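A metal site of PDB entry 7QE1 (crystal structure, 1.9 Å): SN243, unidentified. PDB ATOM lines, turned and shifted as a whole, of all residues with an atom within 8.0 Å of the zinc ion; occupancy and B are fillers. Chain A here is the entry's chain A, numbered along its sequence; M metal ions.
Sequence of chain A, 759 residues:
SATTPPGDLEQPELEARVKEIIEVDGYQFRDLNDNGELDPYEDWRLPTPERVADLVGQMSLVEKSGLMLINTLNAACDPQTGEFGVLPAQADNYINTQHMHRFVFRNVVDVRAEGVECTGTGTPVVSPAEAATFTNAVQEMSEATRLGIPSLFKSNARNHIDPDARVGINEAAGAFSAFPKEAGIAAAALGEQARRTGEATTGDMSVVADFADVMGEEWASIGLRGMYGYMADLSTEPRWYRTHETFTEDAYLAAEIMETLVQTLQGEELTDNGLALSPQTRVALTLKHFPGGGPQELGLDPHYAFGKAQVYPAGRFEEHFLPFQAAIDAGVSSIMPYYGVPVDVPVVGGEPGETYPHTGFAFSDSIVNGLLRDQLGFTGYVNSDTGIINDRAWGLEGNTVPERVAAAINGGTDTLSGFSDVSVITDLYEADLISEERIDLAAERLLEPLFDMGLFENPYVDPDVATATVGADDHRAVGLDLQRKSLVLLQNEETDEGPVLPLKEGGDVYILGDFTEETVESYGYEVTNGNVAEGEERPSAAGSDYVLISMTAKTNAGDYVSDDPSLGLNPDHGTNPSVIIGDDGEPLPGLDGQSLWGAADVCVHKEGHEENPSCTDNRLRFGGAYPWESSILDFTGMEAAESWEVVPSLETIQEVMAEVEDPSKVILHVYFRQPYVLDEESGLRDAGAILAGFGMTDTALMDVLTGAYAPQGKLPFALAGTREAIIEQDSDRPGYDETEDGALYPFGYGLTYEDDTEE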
ATOM      1  N   GLU A  20       0.516  -6.621  27.492  1.00  0.00           N
ATOM      2  CA  GLU A  20      -0.359  -5.438  27.609  1.00  0.00           C
ATOM      3  C   GLU A  20       0.065  -4.418  26.550  1.00  0.00           C
ATOM      4  O   GLU A  20       1.240  -4.384  26.183  1.00  0.00           O
ATOM      5  CB  GLU A  20      -0.263  -4.834  29.006  1.00  0.00           C
ATOM      6  CG  GLU A  20      -0.662  -5.792  30.114  1.00  0.00           C
ATOM      7  CD  GLU A  20      -1.781  -5.288  31.009  1.00  0.00           C
ATOM      8  OE1 GLU A  20      -2.603  -6.116  31.448  1.00  0.00           O
ATOM      9  OE2 GLU A  20      -1.817  -4.068  31.275  1.00  0.00           O
ATOM     10  N   ILE A  22       1.069  -0.818  25.349  1.00  0.00           N
ATOM     11  CA  ILE A  22       1.665   0.389  25.985  1.00  0.00           C
ATOM     12  C   ILE A  22       1.588   1.512  24.969  1.00  0.00           C
ATOM     13  O   ILE A  22       1.689   1.223  23.765  1.00  0.00           O
ATOM     14  CB  ILE A  22       3.115   0.094  26.411  1.00  0.00           C
ATOM     15  CG1 ILE A  22       3.180  -0.722  27.705  1.00  0.00           C
ATOM     16  CG2 ILE A  22       3.928   1.371  26.515  1.00  0.00           C
ATOM     17  CD1 ILE A  22       4.586  -0.923  28.211  1.00  0.00           C
ATOM     18  N   ARG A  30       3.227  -2.955  21.881  1.00  0.00           N
ATOM     19  CA  ARG A  30       3.002  -4.125  22.758  1.00  0.00           C
ATOM     20  C   ARG A  30       4.231  -4.341  23.642  1.00  0.00           C
ATOM     21  O   ARG A  30       5.344  -4.272  23.118  1.00  0.00           O
ATOM     22  CB  ARG A  30       2.734  -5.384  21.925  1.00  0.00           C
ATOM     23  CG  ARG A  30       1.634  -5.248  20.886  1.00  0.00           C
ATOM     24  CD  ARG A  30       1.653  -6.410  19.917  1.00  0.00           C
ATOM     25  NE  ARG A  30       1.178  -7.650  20.509  1.00  0.00           N
ATOM     26  CZ  ARG A  30       1.643  -8.860  20.213  1.00  0.00           C
ATOM     27  NH1 ARG A  30       2.614  -8.991  19.325  1.00  0.00           N
ATOM     28  NH2 ARG A  30       1.144  -9.918  20.804  1.00  0.00           N
ATOM     29  N   ASP A  31       4.021  -4.584  24.934  1.00  0.00           N
ATOM     30  CA  ASP A  31       5.158  -4.849  25.844  1.00  0.00           C
ATOM     31  C   ASP A  31       5.350  -6.363  25.951  1.00  0.00           C
ATOM     32  O   ASP A  31       4.783  -6.967  26.869  1.00  0.00           O
ATOM     33  CB  ASP A  31       4.983  -4.225  27.232  1.00  0.00           C
ATOM     34  CG  ASP A  31       6.320  -3.940  27.893  1.00  0.00           C
ATOM     35  OD1 ASP A  31       7.258  -3.567  27.166  1.00  0.00           O
ATOM     36  OD2 ASP A  31       6.415  -4.101  29.118  1.00  0.00           O
ATOM     37  N   LEU A  32       6.134  -6.919  25.027  1.00  0.00           N
ATOM     38  CA  LEU A  32       6.301  -8.396  24.998  1.00  0.00           C
ATOM     39  C   LEU A  32       7.242  -8.828  26.127  1.00  0.00           C
ATOM     40  O   LEU A  32       7.202 -10.020  26.498  1.00  0.00           O
ATOM     41  CB  LEU A  32       6.840  -8.774  23.618  1.00  0.00           C
ATOM     42  CG  LEU A  32       6.012  -8.277  22.435  1.00  0.00           C
ATOM     43  CD1 LEU A  32       6.746  -8.490  21.123  1.00  0.00           C
ATOM     44  CD2 LEU A  32       4.652  -8.956  22.409  1.00  0.00           C
ATOM     45  N   ASN A  33       8.037  -7.898  26.656  1.00  0.00           N
ATOM     46  CA  ASN A  33       8.974  -8.218  27.772  1.00  0.00           C
ATOM     47  C   ASN A  33       8.294  -7.949  29.120  1.00  0.00           C
ATOM     48  O   ASN A  33       8.811  -8.432  30.137  1.00  0.00           O
ATOM     49  CB  ASN A  33      10.297  -7.451  27.632  1.00  0.00           C
ATOM     50  CG  ASN A  33      10.157  -5.961  27.843  1.00  0.00           C
ATOM     51  OD1 ASN A  33       9.063  -5.406  27.764  1.00  0.00           O
ATOM     52  ND2 ASN A  33      11.271  -5.301  28.106  1.00  0.00           N
ATOM     53  N   ASP A  34       7.180  -7.213  29.116  1.00  0.00           N
ATOM     54  CA  ASP A  34       6.407  -6.944  30.357  1.00  0.00           C
ATOM     55  C   ASP A  34       7.275  -6.164  31.342  1.00  0.00           C
ATOM     56  O   ASP A  34       7.108  -6.354  32.557  1.00  0.00           O
ATOM     57  CB  ASP A  34       5.874  -8.251  30.965  1.00  0.00           C
ATOM     58  CG  ASP A  34       4.690  -8.038  31.892  1.00  0.00           C
ATOM     59  OD1 ASP A  34       4.212  -6.892  31.982  1.00  0.00           O
ATOM     60  OD2 ASP A  34       4.251  -9.022  32.526  1.00  0.00           O
ATOM     61  N   ASN A  35       8.182  -5.322  30.828  1.00  0.00           N
ATOM     62  CA  ASN A  35       9.035  -4.485  31.697  1.00  0.00           C
ATOM     63  C   ASN A  35       8.239  -3.228  32.076  1.00  0.00           C
ATOM     64  O   ASN A  35       8.544  -2.617  33.112  1.00  0.00           O
ATOM     65  CB  ASN A  35      10.343  -4.105  31.021  1.00  0.00           C
ATOM     66  CG  ASN A  35      10.134  -3.271  29.775  1.00  0.00           C
ATOM     67  OD1 ASN A  35       9.037  -3.219  29.227  1.00  0.00           O
ATOM     68  ND2 ASN A  35      11.187  -2.617  29.308  1.00  0.00           N
ATOM     69  N   GLY A  36       7.250  -2.873  31.256  1.00  0.00           N
ATOM     70  CA  GLY A  36       6.474  -1.639  31.491  1.00  0.00           C
ATOM     71  C   GLY A  36       7.031  -0.517  30.662  1.00  0.00           C
ATOM     72  O   GLY A  36       6.499   0.601  30.730  1.00  0.00           O
ATOM     73  N   GLU A  37       8.087  -0.803  29.896  1.00  0.00           N
ATOM     74  CA  GLU A  37       8.754   0.249  29.083  1.00  0.00           C
ATOM     75  C   GLU A  37       8.788  -0.189  27.625  1.00  0.00           C
ATOM     76  O   GLU A  37       8.806  -1.408  27.370  1.00  0.00           O
ATOM     77  CB  GLU A  37      10.166   0.482  29.594  1.00  0.00           C
ATOM     78  CG  GLU A  37      10.210   1.095  30.987  1.00  0.00           C
ATOM     79  CD  GLU A  37      11.607   1.267  31.569  1.00  0.00           C
ATOM     80  OE1 GLU A  37      12.564   0.748  30.964  1.00  0.00           O
ATOM     81  OE2 GLU A  37      11.727   1.928  32.616  1.00  0.00           O
ATOM     82  N   LEU A  38       8.808   0.768  26.691  1.00  0.00           N
ATOM     83  CA  LEU A  38       8.894   0.429  25.254  1.00  0.00           C
ATOM     84  C   LEU A  38      10.348   0.118  24.919  1.00  0.00           C
ATOM     85  O   LEU A  38      11.114   1.073  24.676  1.00  0.00           O
ATOM     86  CB  LEU A  38       8.389   1.600  24.416  1.00  0.00           C
ATOM     87  CG  LEU A  38       8.515   1.418  22.907  1.00  0.00           C
ATOM     88  CD1 LEU A  38       7.782   0.169  22.446  1.00  0.00           C
ATOM     89  CD2 LEU A  38       7.997   2.635  22.157  1.00  0.00           C
ATOM     90  N   ASP A  39      10.723  -1.163  24.927  1.00  0.00           N
ATOM     91  CA  ASP A  39      12.092  -1.531  24.504  1.00  0.00           C
ATOM     92  C   ASP A  39      12.178  -1.361  22.986  1.00  0.00           C
ATOM     93  O   ASP A  39      11.152  -1.580  22.317  1.00  0.00           O
ATOM     94  CB  ASP A  39      12.446  -2.937  24.984  1.00  0.00           C
ATOM     95  CG  ASP A  39      11.967  -3.208  26.398  1.00  0.00           C
ATOM     96  OD1 ASP A  39      10.737  -3.157  26.621  1.00  0.00           O
ATOM     97  OD2 ASP A  39      12.822  -3.466  27.261  1.00  0.00           O
ATOM     98  N   PRO A  40      13.338  -0.977  22.419  1.00  0.00           N
ATOM     99  CA  PRO A  40      13.427  -0.696  20.986  1.00  0.00           C
ATOM    100  C   PRO A  40      12.842  -1.796  20.078  1.00  0.00           C
ATOM    101  O   PRO A  40      12.230  -1.457  19.097  1.00  0.00           O
ATOM    102  CB  PRO A  40      14.938  -0.572  20.765  1.00  0.00           C
ATOM    103  CG  PRO A  40      15.464  -0.076  22.088  1.00  0.00           C
ATOM    104  CD  PRO A  40      14.597  -0.776  23.122  1.00  0.00           C
ATOM    105  N   TYR A  41      13.051  -3.069  20.430  1.00  0.00           N
ATOM    106  CA  TYR A  41      12.587  -4.164  19.541  1.00  0.00           C
ATOM    107  C   TYR A  41      11.057  -4.153  19.506  1.00  0.00           C
ATOM    108  O   TYR A  41      10.470  -4.682  18.535  1.00  0.00           O
ATOM    109  CB  TYR A  41      13.178  -5.515  19.969  1.00  0.00           C
ATOM    110  CG  TYR A  41      12.464  -6.217  21.092  1.00  0.00           C
ATOM    111  CD1 TYR A  41      11.435  -7.108  20.838  1.00  0.00           C
ATOM    112  CD2 TYR A  41      12.852  -6.029  22.411  1.00  0.00           C
ATOM    113  CE1 TYR A  41      10.788  -7.768  21.867  1.00  0.00           C
ATOM    114  CE2 TYR A  41      12.209  -6.685  23.453  1.00  0.00           C
ATOM    115  CZ  TYR A  41      11.178  -7.563  23.172  1.00  0.00           C
ATOM    116  OH  TYR A  41      10.544  -8.213  24.194  1.00  0.00           O
ATOM    117  N   GLU A  42      10.425  -3.572  20.532  1.00  0.00           N
ATOM    118  CA  GLU A  42       8.940  -3.486  20.574  1.00  0.00           C
ATOM    119  C   GLU A  42       8.502  -2.236  19.814  1.00  0.00           C
ATOM    120  O   GLU A  42       7.288  -1.986  19.764  1.00  0.00           O
ATOM    121  CB  GLU A  42       8.481  -3.400  22.023  1.00  0.00           C
ATOM    122  CG  GLU A  42       9.071  -4.460  22.931  1.00  0.00           C
ATOM    123  CD  GLU A  42       8.759  -4.276  24.406  1.00  0.00           C
ATOM    124  OE1 GLU A  42       8.652  -3.121  24.845  1.00  0.00           O
ATOM    125  OE2 GLU A  42       8.606  -5.299  25.105  1.00  0.00           O
ATOM    126  N   ASP A  54      18.414  -5.040  19.316  1.00  0.00           N
ATOM    127  CA  ASP A  54      17.927  -4.848  20.683  1.00  0.00           C
ATOM    128  C   ASP A  54      17.377  -6.133  21.280  1.00  0.00           C
ATOM    129  O   ASP A  54      17.473  -6.360  22.496  1.00  0.00           O
ATOM    130  CB  ASP A  54      16.874  -3.732  20.733  1.00  0.00           C
ATOM    131  CG  ASP A  54      16.312  -3.533  22.141  1.00  0.00           C
ATOM    132  OD1 ASP A  54      17.069  -3.099  23.035  1.00  0.00           O
ATOM    133  OD2 ASP A  54      15.122  -3.822  22.345  1.00  0.00           O
ATOM    134  N   GLN A  58      18.990  -9.054  24.422  1.00  0.00           N
ATOM    135  CA  GLN A  58      18.244  -9.387  25.622  1.00  0.00           C
ATOM    136  C   GLN A  58      18.015 -10.886  25.824  1.00  0.00           C
ATOM    137  O   GLN A  58      17.457 -11.269  26.858  1.00  0.00           O
ATOM    138  CB  GLN A  58      16.864  -8.693  25.613  1.00  0.00           C
ATOM    139  CG  GLN A  58      16.880  -7.213  25.313  1.00  0.00           C
ATOM    140  CD  GLN A  58      15.495  -6.611  25.360  1.00  0.00           C
ATOM    141  OE1 GLN A  58      14.616  -7.103  26.072  1.00  0.00           O
ATOM    142  NE2 GLN A  58      15.284  -5.536  24.605  1.00  0.00           N
ATOM    143  N   ARG A 146       8.754 -14.976  27.932  1.00  0.00           N
ATOM    144  CA  ARG A 146       9.407 -13.774  28.485  1.00  0.00           C
ATOM    145  C   ARG A 146       9.454 -12.658  27.459  1.00  0.00           C
ATOM    146  O   ARG A 146       8.973 -11.582  27.759  1.00  0.00           O
ATOM    147  CB  ARG A 146      10.819 -14.147  28.932  1.00  0.00           C
ATOM    148  CG  ARG A 146      11.697 -12.973  29.316  1.00  0.00           C
ATOM    149  CD  ARG A 146      12.889 -13.433  30.132  1.00  0.00           C
ATOM    150  NE  ARG A 146      14.042 -13.698  29.293  1.00  0.00           N
ATOM    151  CZ  ARG A 146      14.816 -12.756  28.766  1.00  0.00           C
ATOM    152  NH1 ARG A 146      14.555 -11.483  28.992  1.00  0.00           N
ATOM    153  NH2 ARG A 146      15.851 -13.086  28.013  1.00  0.00           N
HETATM  154 ZN    ZN M   1       9.064  -3.663  27.047  1.00  0.00          ZN
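Six residues have an atom within 4 Å of the zinc ion: Asp 31, Asn 33, Asn 35, Glu 37, Asp 39 and Glu 42.
The zinc ion is bound by the side-chain carboxylate (OD1) of Asp 39 (1.8 Å), the side-chain carboxylate (OD1) of Asp 31 (1.8 Å), the side-chain amide oxygen (OD1) of Asn 33 (1.9 Å), the side-chain amide oxygen (OD1) of Asn 35 (2.2 Å), the backbone carbonyl oxygen (O) of Glu 37 (2.3 Å), the side-chain carboxylate (OE1) of Glu 42 (2.3 Å) and the side-chain carboxylate (OE2) of Glu 42 (2.6 Å).
The side-chain carboxylate (OE2) of Glu 42 lies close to the backbone NH (N) of Leu 32 (3.0 Å).
N of Asp 31 is in hydrogen-bond range of O of Glu 20, at 3.1 Å.
OD2 of Asp 31 lies close to N of Asp 34 (3.2 Å).
The side-chain carboxylate (OD2) of Asp 31 is in hydrogen-bond range of the backbone NH (N) of Gly 36, 2.6 Å away.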
